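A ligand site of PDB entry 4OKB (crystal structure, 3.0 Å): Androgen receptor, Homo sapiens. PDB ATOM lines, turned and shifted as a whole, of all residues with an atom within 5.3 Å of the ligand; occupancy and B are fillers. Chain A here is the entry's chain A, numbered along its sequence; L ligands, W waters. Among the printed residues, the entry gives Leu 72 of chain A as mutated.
An oxygen (O3) of the ligand sits close to the backbone NH (N) of Asn 36, at 3.1 Å. OD1 of Asn 36 sits at hydrogen-bond distance from O3 of the ligand (2.7 Å). NH2 of Arg 83 sits at hydrogen-bond distance from N2 of the ligand (3.0 Å). O of Leu 35 is in hydrogen-bond range of O3 of the ligand. The side-chain amide oxygen (OE1) of Gln 42 lies close to a nitrogen (N2) of the ligand (3.4 Å).
ND2 of Asn 36 sits close to O of Leu 32, 3.0 Å away. The side-chain sulfur (SD) of Met 76 lies close to the side-chain amide nitrogen (NE2) of Gln 42 (3.5 Å). The guanidinium group (NH2) of Arg 83 lies within hydrogen-bond range of the backbone carbonyl oxygen (O) of Phe 95, at 3.2 Å. O of Tyr 94 is in hydrogen-bond range of NE of Arg 83. O of Leu 204 lies within hydrogen-bond range of OG1 of Thr 208 (2.8 Å). The backbone NH (N) of Val 234 lies within hydrogen-bond range of the backbone carbonyl oxygen (O) of Ile 229, at 3.3 Å.
SD of Met 73 sits close to O4 of the ligand, 3.5 Å away. The backbone carbonyl oxygen (O) of Met 76 lies close to a fluorine (F3) of the ligand, 3.2 Å away. N of Val 77 sits close to F3 of the ligand (2.9 Å). NE2 of His 205 lies close to F1 of the ligand. Merely in contact with the ligand: Met 80 (3.1 Å), Gly 39 (3.2 Å), Leu 204 (3.5 Å), Thr 208 (3.5 Å), Ile 230 (3.6 Å), Leu 72 (3.6 Å), Phe 95 (3.6 Å), Gln 69 (3.6 Å), Leu 38 (3.7 Å), Met 226 (3.7 Å), Val 234 (3.9 Å) and Met 118 (3.97 Å). Hydrophobic or aromatic side chains within 4 Å of the ligand: Leu 35, Leu 38, Leu 72, Met 73, Met 76, Val 77, Met 80, Phe 95, Met 118, Leu 204, His 205, Met 226, Ile 230 and Val 234. Within 4 Å of the ligand: Leu 35, Asn 36, Leu 38, Gly 39, Gln 42, Gln 69, Leu 72, Met 73, Met 76, Val 77, Met 80, Arg 83, Phe 95, Met 118, Leu 204, His 205, Thr 208, Met 226, Ile 230 and Val 234.
Water W1 lies within hydrogen-bond range of the guanidinium group (NH2) of Arg 83 (2.6 Å), the side-chain amide nitrogen (NE2) of Gln 42 (2.7 Å), the backbone carbonyl oxygen (O) of Met 76 (3.0 Å) and a nitrogen (N2) of the ligand (3.1 Å).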
ATOM      1  N   LEU A  32       4.759  19.927  17.860  1.00  0.00           N
ATOM      2  CA  LEU A  32       5.348  19.328  16.679  1.00  0.00           C
ATOM      3  C   LEU A  32       4.638  19.652  15.403  1.00  0.00           C
ATOM      4  O   LEU A  32       5.293  19.723  14.366  1.00  0.00           O
ATOM      5  CB  LEU A  32       5.581  17.842  16.838  1.00  0.00           C
ATOM      6  CG  LEU A  32       6.961  17.781  17.539  1.00  0.00           C
ATOM      7  CD1 LEU A  32       6.831  17.618  19.048  1.00  0.00           C
ATOM      8  CD2 LEU A  32       7.842  16.707  16.954  1.00  0.00           C
ATOM      9  N   LEU A  35       6.578  22.796  14.802  1.00  0.00           N
ATOM     10  CA  LEU A  35       7.932  22.539  14.307  1.00  0.00           C
ATOM     11  C   LEU A  35       7.956  22.141  12.834  1.00  0.00           C
ATOM     12  O   LEU A  35       8.855  22.590  12.103  1.00  0.00           O
ATOM     13  CB  LEU A  35       8.620  21.464  15.143  1.00  0.00           C
ATOM     14  CG  LEU A  35       9.204  22.096  16.422  1.00  0.00           C
ATOM     15  CD1 LEU A  35       9.698  21.041  17.404  1.00  0.00           C
ATOM     16  CD2 LEU A  35      10.327  23.064  16.045  1.00  0.00           C
ATOM     17  N   ASN A  36       6.973  21.343  12.411  1.00  0.00           N
ATOM     18  CA  ASN A  36       6.862  20.879  11.014  1.00  0.00           C
ATOM     19  C   ASN A  36       6.570  21.991  10.069  1.00  0.00           C
ATOM     20  O   ASN A  36       7.145  22.017   8.977  1.00  0.00           O
ATOM     21  CB  ASN A  36       5.791  19.802  10.869  1.00  0.00           C
ATOM     22  CG  ASN A  36       6.073  18.595  11.707  1.00  0.00           C
ATOM     23  OD1 ASN A  36       7.194  18.368  12.075  1.00  0.00           O
ATOM     24  ND2 ASN A  36       5.051  17.823  12.018  1.00  0.00           N
ATOM     25  N   GLU A  37       5.689  22.917  10.474  1.00  0.00           N
ATOM     26  CA  GLU A  37       5.330  24.077   9.643  1.00  0.00           C
ATOM     27  C   GLU A  37       6.540  24.998   9.499  1.00  0.00           C
ATOM     28  O   GLU A  37       6.824  25.520   8.427  1.00  0.00           O
ATOM     29  CB  GLU A  37       4.152  24.879  10.229  1.00  0.00           C
ATOM     30  CG  GLU A  37       3.572  25.937   9.281  1.00  0.00           C
ATOM     31  CD  GLU A  37       2.999  25.366   7.965  1.00  0.00           C
ATOM     32  OE1 GLU A  37       3.062  26.056   6.905  1.00  0.00           O
ATOM     33  OE2 GLU A  37       2.484  24.220   7.993  1.00  0.00           O
ATOM     34  N   LEU A  38       7.231  25.176  10.602  1.00  0.00           N
ATOM     35  CA  LEU A  38       8.464  25.907  10.591  1.00  0.00           C
ATOM     36  C   LEU A  38       9.493  25.248   9.670  1.00  0.00           C
ATOM     37  O   LEU A  38      10.315  25.947   9.065  1.00  0.00           O
ATOM     38  CB  LEU A  38       9.009  25.979  12.017  1.00  0.00           C
ATOM     39  CG  LEU A  38      10.200  26.904  12.123  1.00  0.00           C
ATOM     40  CD1 LEU A  38       9.888  28.264  11.542  1.00  0.00           C
ATOM     41  CD2 LEU A  38      10.601  27.000  13.578  1.00  0.00           C
ATOM     42  N   GLY A  39       9.439  23.915   9.580  1.00  0.00           N
ATOM     43  CA  GLY A  39      10.350  23.144   8.759  1.00  0.00           C
ATOM     44  C   GLY A  39      10.204  23.628   7.346  1.00  0.00           C
ATOM     45  O   GLY A  39      11.149  24.097   6.718  1.00  0.00           O
ATOM     46  N   GLU A  40       8.965  23.560   6.887  1.00  0.00           N
ATOM     47  CA  GLU A  40       8.618  23.953   5.533  1.00  0.00           C
ATOM     48  C   GLU A  40       8.953  25.424   5.249  1.00  0.00           C
ATOM     49  O   GLU A  40       9.510  25.757   4.204  1.00  0.00           O
ATOM     50  CB  GLU A  40       7.133  23.704   5.279  1.00  0.00           C
ATOM     51  CG  GLU A  40       6.757  23.783   3.818  1.00  0.00           C
ATOM     52  CD  GLU A  40       5.284  23.561   3.622  1.00  0.00           C
ATOM     53  OE1 GLU A  40       4.930  22.457   3.118  1.00  0.00           O
ATOM     54  OE2 GLU A  40       4.475  24.477   4.000  1.00  0.00           O
ATOM     55  N   GLN A  42      11.164  27.260   6.734  1.00  0.00           N
ATOM     56  CA  GLN A  42      12.629  27.372   6.673  1.00  0.00           C
ATOM     57  C   GLN A  42      13.167  26.747   5.400  1.00  0.00           C
ATOM     58  O   GLN A  42      14.012  27.330   4.761  1.00  0.00           O
ATOM     59  CB  GLN A  42      13.307  26.840   7.951  1.00  0.00           C
ATOM     60  CG  GLN A  42      13.145  27.775   9.147  1.00  0.00           C
ATOM     61  CD  GLN A  42      13.912  27.314  10.392  1.00  0.00           C
ATOM     62  OE1 GLN A  42      13.525  27.618  11.521  1.00  0.00           O
ATOM     63  NE2 GLN A  42      15.008  26.576  10.181  1.00  0.00           N
ATOM     64  N   GLN A  69      17.925  18.676   0.284  1.00  0.00           N
ATOM     65  CA  GLN A  69      17.051  17.865   1.100  1.00  0.00           C
ATOM     66  C   GLN A  69      17.854  17.126   2.193  1.00  0.00           C
ATOM     67  O   GLN A  69      17.427  16.992   3.355  1.00  0.00           O
ATOM     68  CB  GLN A  69      16.279  16.946   0.201  1.00  0.00           C
ATOM     69  CG  GLN A  69      15.258  17.722  -0.621  1.00  0.00           C
ATOM     70  CD  GLN A  69      14.603  16.883  -1.694  1.00  0.00           C
ATOM     71  OE1 GLN A  69      15.172  16.631  -2.770  1.00  0.00           O
ATOM     72  NE2 GLN A  69      13.405  16.433  -1.408  1.00  0.00           N
ATOM     73  N   TYR A  70      19.048  16.714   1.824  1.00  0.00           N
ATOM     74  CA  TYR A  70      19.905  16.024   2.740  1.00  0.00           C
ATOM     75  C   TYR A  70      20.365  16.951   3.840  1.00  0.00           C
ATOM     76  O   TYR A  70      20.183  16.660   5.027  1.00  0.00           O
ATOM     77  CB  TYR A  70      21.095  15.447   1.968  1.00  0.00           C
ATOM     78  CG  TYR A  70      20.699  14.499   0.840  1.00  0.00           C
ATOM     79  CD1 TYR A  70      19.547  13.696   0.931  1.00  0.00           C
ATOM     80  CD2 TYR A  70      21.480  14.386  -0.305  1.00  0.00           C
ATOM     81  CE1 TYR A  70      19.188  12.817  -0.067  1.00  0.00           C
ATOM     82  CE2 TYR A  70      21.134  13.490  -1.326  1.00  0.00           C
ATOM     83  CZ  TYR A  70      19.977  12.706  -1.207  1.00  0.00           C
ATOM     84  OH  TYR A  70      19.604  11.803  -2.218  1.00  0.00           O
ATOM     85  N   LEU A  72      19.131  19.828   4.777  1.00  0.00           N
ATOM     86  CA  LEU A  72      18.141  20.680   5.407  1.00  0.00           C
ATOM     87  C   LEU A  72      18.216  20.688   6.919  1.00  0.00           C
ATOM     88  O   LEU A  72      18.331  21.745   7.517  1.00  0.00           O
ATOM     89  CB  LEU A  72      16.727  20.284   4.990  1.00  0.00           C
ATOM     90  CG  LEU A  72      15.701  21.158   5.724  1.00  0.00           C
ATOM     91  CD1 LEU A  72      15.988  22.617   5.428  1.00  0.00           C
ATOM     92  CD2 LEU A  72      14.279  20.806   5.312  1.00  0.00           C
ATOM     93  N   MET A  73      18.149  19.521   7.544  1.00  0.00           N
ATOM     94  CA  MET A  73      18.134  19.436   9.011  1.00  0.00           C
ATOM     95  C   MET A  73      19.345  20.152   9.604  1.00  0.00           C
ATOM     96  O   MET A  73      19.180  21.073  10.444  1.00  0.00           O
ATOM     97  CB  MET A  73      18.076  17.966   9.501  1.00  0.00           C
ATOM     98  CG  MET A  73      17.645  17.816  10.954  1.00  0.00           C
ATOM     99  SD  MET A  73      15.977  18.440  11.283  1.00  0.00           S
ATOM    100  CE  MET A  73      15.082  17.001  10.722  1.00  0.00           C
ATOM    101  N   MET A  76      19.238  23.842   9.379  1.00  0.00           N
ATOM    102  CA  MET A  76      18.262  24.346  10.345  1.00  0.00           C
ATOM    103  C   MET A  76      18.842  24.332  11.770  1.00  0.00           C
ATOM    104  O   MET A  76      18.696  25.271  12.568  1.00  0.00           O
ATOM    105  CB  MET A  76      17.000  23.495  10.269  1.00  0.00           C
ATOM    106  CG  MET A  76      16.230  23.668   8.972  1.00  0.00           C
ATOM    107  SD  MET A  76      14.478  23.270   9.128  1.00  0.00           S
ATOM    108  CE  MET A  76      14.651  21.568   9.669  1.00  0.00           C
ATOM    109  N   VAL A  77      19.534  23.248  12.061  1.00  0.00           N
ATOM    110  CA  VAL A  77      20.101  23.031  13.365  1.00  0.00           C
ATOM    111  C   VAL A  77      21.192  24.032  13.641  1.00  0.00           C
ATOM    112  O   VAL A  77      21.218  24.644  14.690  1.00  0.00           O
ATOM    113  CB  VAL A  77      20.716  21.629  13.428  1.00  0.00           C
ATOM    114  CG1 VAL A  77      21.606  21.505  14.658  1.00  0.00           C
ATOM    115  CG2 VAL A  77      19.604  20.575  13.419  1.00  0.00           C
ATOM    116  N   MET A  80      19.881  27.596  13.870  1.00  0.00           N
ATOM    117  CA  MET A  80      19.106  27.700  15.092  1.00  0.00           C
ATOM    118  C   MET A  80      20.026  27.911  16.291  1.00  0.00           C
ATOM    119  O   MET A  80      19.772  28.800  17.091  1.00  0.00           O
ATOM    120  CB  MET A  80      18.219  26.469  15.282  1.00  0.00           C
ATOM    121  CG  MET A  80      17.285  26.585  16.457  1.00  0.00           C
ATOM    122  SD  MET A  80      18.042  26.018  18.005  1.00  0.00           S
ATOM    123  CE  MET A  80      16.957  24.610  18.247  1.00  0.00           C
ATOM    124  N   ARG A  83      21.296  31.593  16.222  1.00  0.00           N
ATOM    125  CA  ARG A  83      20.133  32.404  16.563  1.00  0.00           C
ATOM    126  C   ARG A  83      19.948  32.383  18.055  1.00  0.00           C
ATOM    127  O   ARG A  83      19.806  33.400  18.699  1.00  0.00           O
ATOM    128  CB  ARG A  83      18.868  31.814  15.935  1.00  0.00           C
ATOM    129  CG  ARG A  83      18.107  32.793  15.088  1.00  0.00           C
ATOM    130  CD  ARG A  83      16.667  32.386  14.767  1.00  0.00           C
ATOM    131  NE  ARG A  83      16.391  30.955  14.605  1.00  0.00           N
ATOM    132  CZ  ARG A  83      16.809  30.194  13.594  1.00  0.00           C
ATOM    133  NH1 ARG A  83      17.601  30.665  12.651  1.00  0.00           N
ATOM    134  NH2 ARG A  83      16.451  28.926  13.548  1.00  0.00           N
ATOM    135  N   TYR A  94      15.913  29.003  20.370  1.00  0.00           N
ATOM    136  CA  TYR A  94      15.218  30.011  19.587  1.00  0.00           C
ATOM    137  C   TYR A  94      14.909  29.475  18.172  1.00  0.00           C
ATOM    138  O   TYR A  94      15.457  29.922  17.157  1.00  0.00           O
ATOM    139  CB  TYR A  94      16.072  31.275  19.536  1.00  0.00           C
ATOM    140  CG  TYR A  94      15.308  32.562  19.353  1.00  0.00           C
ATOM    141  CD1 TYR A  94      14.863  32.967  18.094  1.00  0.00           C
ATOM    142  CD2 TYR A  94      15.064  33.399  20.426  1.00  0.00           C
ATOM    143  CE1 TYR A  94      14.191  34.156  17.912  1.00  0.00           C
ATOM    144  CE2 TYR A  94      14.387  34.591  20.252  1.00  0.00           C
ATOM    145  CZ  TYR A  94      13.955  34.966  18.998  1.00  0.00           C
ATOM    146  OH  TYR A  94      13.273  36.161  18.833  1.00  0.00           O
ATOM    147  N   PHE A  95      14.015  28.504  18.118  1.00  0.00           N
ATOM    148  CA  PHE A  95      13.610  27.977  16.861  1.00  0.00           C
ATOM    149  C   PHE A  95      13.088  29.116  15.979  1.00  0.00           C
ATOM    150  O   PHE A  95      13.476  29.248  14.806  1.00  0.00           O
ATOM    151  CB  PHE A  95      12.547  26.928  17.082  1.00  0.00           C
ATOM    152  CG  PHE A  95      13.045  25.669  17.738  1.00  0.00           C
ATOM    153  CD1 PHE A  95      13.070  25.545  19.120  1.00  0.00           C
ATOM    154  CD2 PHE A  95      13.428  24.588  16.979  1.00  0.00           C
ATOM    155  CE1 PHE A  95      13.496  24.375  19.718  1.00  0.00           C
ATOM    156  CE2 PHE A  95      13.842  23.413  17.559  1.00  0.00           C
ATOM    157  CZ  PHE A  95      13.872  23.306  18.927  1.00  0.00           C
ATOM    158  N   MET A 118      21.652  20.313  21.183  1.00  0.00           N
ATOM    159  CA  MET A 118      21.538  21.554  20.406  1.00  0.00           C
ATOM    160  C   MET A 118      21.822  22.785  21.247  1.00  0.00           C
ATOM    161  O   MET A 118      22.492  23.715  20.767  1.00  0.00           O
ATOM    162  CB  MET A 118      20.120  21.688  19.804  1.00  0.00           C
ATOM    163  CG  MET A 118      19.803  20.755  18.631  1.00  0.00           C
ATOM    164  SD  MET A 118      18.145  21.031  17.953  1.00  0.00           S
ATOM    165  CE  MET A 118      17.098  20.212  19.139  1.00  0.00           C
ATOM    166  N   LEU A 204      17.657  13.812  14.875  1.00  0.00           N
ATOM    167  CA  LEU A 204      16.473  14.548  14.522  1.00  0.00           C
ATOM    168  C   LEU A 204      15.790  13.816  13.388  1.00  0.00           C
ATOM    169  O   LEU A 204      14.585  13.582  13.420  1.00  0.00           O
ATOM    170  CB  LEU A 204      16.815  15.988  14.169  1.00  0.00           C
ATOM    171  CG  LEU A 204      17.077  16.810  15.453  1.00  0.00           C
ATOM    172  CD1 LEU A 204      17.681  18.164  15.121  1.00  0.00           C
ATOM    173  CD2 LEU A 204      15.805  16.989  16.283  1.00  0.00           C
ATOM    174  N   HIS A 205      16.584  13.402  12.420  1.00  0.00           N
ATOM    175  CA  HIS A 205      16.054  12.689  11.295  1.00  0.00           C
ATOM    176  C   HIS A 205      15.350  11.451  11.723  1.00  0.00           C
ATOM    177  O   HIS A 205      14.296  11.133  11.187  1.00  0.00           O
ATOM    178  CB  HIS A 205      17.168  12.342  10.309  1.00  0.00           C
ATOM    179  CG  HIS A 205      17.345  13.367   9.230  1.00  0.00           C
ATOM    180  ND1 HIS A 205      18.590  13.741   8.768  1.00  0.00           N
ATOM    181  CD2 HIS A 205      16.439  14.098   8.547  1.00  0.00           C
ATOM    182  CE1 HIS A 205      18.442  14.647   7.815  1.00  0.00           C
ATOM    183  NE2 HIS A 205      17.150  14.882   7.659  1.00  0.00           N
ATOM    184  N   PHE A 207      14.019  10.674  14.766  1.00  0.00           N
ATOM    185  CA  PHE A 207      12.820  11.065  15.474  1.00  0.00           C
ATOM    186  C   PHE A 207      11.650  11.473  14.529  1.00  0.00           C
ATOM    187  O   PHE A 207      10.479  11.074  14.707  1.00  0.00           O
ATOM    188  CB  PHE A 207      13.220  12.231  16.390  1.00  0.00           C
ATOM    189  CG  PHE A 207      12.072  12.894  17.039  1.00  0.00           C
ATOM    190  CD1 PHE A 207      11.600  12.453  18.252  1.00  0.00           C
ATOM    191  CD2 PHE A 207      11.448  13.957  16.411  1.00  0.00           C
ATOM    192  CE1 PHE A 207      10.494  13.070  18.856  1.00  0.00           C
ATOM    193  CE2 PHE A 207      10.356  14.566  16.989  1.00  0.00           C
ATOM    194  CZ  PHE A 207       9.875  14.130  18.219  1.00  0.00           C
ATOM    195  N   THR A 208      12.020  12.291  13.544  1.00  0.00           N
ATOM    196  CA  THR A 208      11.110  12.919  12.593  1.00  0.00           C
ATOM    197  C   THR A 208      10.434  11.848  11.787  1.00  0.00           C
ATOM    198  O   THR A 208       9.218  11.840  11.633  1.00  0.00           O
ATOM    199  CB  THR A 208      11.877  13.849  11.606  1.00  0.00           C
ATOM    200  OG1 THR A 208      12.479  14.957  12.286  1.00  0.00           O
ATOM    201  CG2 THR A 208      10.951  14.401  10.575  1.00  0.00           C
ATOM    202  N   PHE A 222       1.669  17.102   9.397  1.00  0.00           N
ATOM    203  CA  PHE A 222       2.791  17.273   8.464  1.00  0.00           C
ATOM    204  C   PHE A 222       2.316  17.897   7.165  1.00  0.00           C
ATOM    205  O   PHE A 222       1.434  17.334   6.496  1.00  0.00           O
ATOM    206  CB  PHE A 222       3.429  15.919   8.106  1.00  0.00           C
ATOM    207  CG  PHE A 222       4.364  15.404   9.154  1.00  0.00           C
ATOM    208  CD1 PHE A 222       5.702  15.800   9.156  1.00  0.00           C
ATOM    209  CD2 PHE A 222       3.912  14.560  10.149  1.00  0.00           C
ATOM    210  CE1 PHE A 222       6.573  15.340  10.138  1.00  0.00           C
ATOM    211  CE2 PHE A 222       4.770  14.101  11.135  1.00  0.00           C
ATOM    212  CZ  PHE A 222       6.103  14.485  11.127  1.00  0.00           C
ATOM    213  N   MET A 226       6.719  18.113   3.296  1.00  0.00           N
ATOM    214  CA  MET A 226       7.679  17.593   4.299  1.00  0.00           C
ATOM    215  C   MET A 226       7.490  16.081   4.465  1.00  0.00           C
ATOM    216  O   MET A 226       8.474  15.329   4.469  1.00  0.00           O
ATOM    217  CB  MET A 226       7.575  18.374   5.615  1.00  0.00           C
ATOM    218  CG  MET A 226       7.769  19.884   5.441  1.00  0.00           C
ATOM    219  SD  MET A 226       9.180  20.407   4.392  1.00  0.00           S
ATOM    220  CE  MET A 226      10.529  20.259   5.558  1.00  0.00           C
ATOM    221  N   ILE A 229       9.206  14.395   1.552  1.00  0.00           N
ATOM    222  CA  ILE A 229      10.662  14.424   1.765  1.00  0.00           C
ATOM    223  C   ILE A 229      11.095  13.400   2.810  1.00  0.00           C
ATOM    224  O   ILE A 229      12.033  12.627   2.603  1.00  0.00           O
ATOM    225  CB  ILE A 229      11.150  15.837   2.198  1.00  0.00           C
ATOM    226  CG1 ILE A 229      11.040  16.832   1.023  1.00  0.00           C
ATOM    227  CG2 ILE A 229      12.570  15.770   2.780  1.00  0.00           C
ATOM    228  CD1 ILE A 229      11.502  18.243   1.310  1.00  0.00           C
ATOM    229  N   ILE A 230      10.393  13.401   3.940  1.00  0.00           N
ATOM    230  CA  ILE A 230      10.652  12.439   4.997  1.00  0.00           C
ATOM    231  C   ILE A 230      10.510  10.982   4.525  1.00  0.00           C
ATOM    232  O   ILE A 230      11.259  10.091   4.942  1.00  0.00           O
ATOM    233  CB  ILE A 230       9.708  12.713   6.175  1.00  0.00           C
ATOM    234  CG1 ILE A 230      10.145  14.009   6.904  1.00  0.00           C
ATOM    235  CG2 ILE A 230       9.702  11.523   7.143  1.00  0.00           C
ATOM    236  CD1 ILE A 230       9.041  14.696   7.702  1.00  0.00           C
ATOM    237  N   VAL A 234      14.874  11.167   3.467  1.00  0.00           N
ATOM    238  CA  VAL A 234      15.365  10.846   4.833  1.00  0.00           C
ATOM    239  C   VAL A 234      15.700   9.360   5.037  1.00  0.00           C
ATOM    240  O   VAL A 234      16.720   9.057   5.659  1.00  0.00           O
ATOM    241  CB  VAL A 234      14.375  11.314   5.921  1.00  0.00           C
ATOM    242  CG1 VAL A 234      14.804  10.810   7.299  1.00  0.00           C
ATOM    243  CG2 VAL A 234      14.284  12.842   5.914  1.00  0.00           C
HETATM  244  C1  LIG L   1      13.252  18.673   8.501  1.00  0.00           C
HETATM  245  C2  LIG L   1      14.265  18.157   7.703  1.00  0.00           C
HETATM  246  C3  LIG L   1      14.015  17.125   6.794  1.00  0.00           C
HETATM  247  F1  LIG L   1      15.020  16.633   6.007  1.00  0.00           F
HETATM  248  C4  LIG L   1      12.738  16.616   6.706  1.00  0.00           C
HETATM  249  C5  LIG L   1      11.729  17.136   7.516  1.00  0.00           C
HETATM  250  C6  LIG L   1      11.975  18.174   8.410  1.00  0.00           C
HETATM  251  S1  LIG L   1      10.813  18.754   9.365  1.00  0.00           S
HETATM  252  O1  LIG L   1      11.073  20.162   9.585  1.00  0.00           O
HETATM  253  O2  LIG L   1       9.505  18.612   8.795  1.00  0.00           O
HETATM  254  C7  LIG L   1      10.866  17.905  10.806  1.00  0.00           C
HETATM  255  C8  LIG L   1      10.576  18.795  12.016  1.00  0.00           C
HETATM  256  O3  LIG L   1       9.485  19.619  11.617  1.00  0.00           O
HETATM  257  C9  LIG L   1      10.155  17.991  13.243  1.00  0.00           C
HETATM  258  C10 LIG L   1      11.765  19.641  12.446  1.00  0.00           C
HETATM  259  O4  LIG L   1      12.812  19.088  12.733  1.00  0.00           O
HETATM  260  N1  LIG L   1      11.557  20.973  12.471  1.00  0.00           N
HETATM  261  C11 LIG L   1      12.476  21.947  12.777  1.00  0.00           C
HETATM  262  C12 LIG L   1      13.762  21.707  13.291  1.00  0.00           C
HETATM  263  C13 LIG L   1      12.097  23.267  12.505  1.00  0.00           C
HETATM  264  C14 LIG L   1      12.945  24.333  12.729  1.00  0.00           C
HETATM  265  C15 LIG L   1      14.214  24.129  13.222  1.00  0.00           C
HETATM  266  C16 LIG L   1      14.972  25.142  13.435  1.00  0.00           C
HETATM  267  N2  LIG L   1      15.669  26.037  13.664  1.00  0.00           N
HETATM  268  C17 LIG L   1      14.654  22.743  13.526  1.00  0.00           C
HETATM  269  C18 LIG L   1      16.045  22.439  14.048  1.00  0.00           C
HETATM  270  F2  LIG L   1      16.015  21.165  14.395  1.00  0.00           F
HETATM  271  F3  LIG L   1      16.922  22.663  13.090  1.00  0.00           F
HETATM  272  F4  LIG L   1      16.427  23.171  15.083  1.00  0.00           F
HETATM  273  O   HOH W   1      17.176  27.568  11.435  1.00  0.00           O
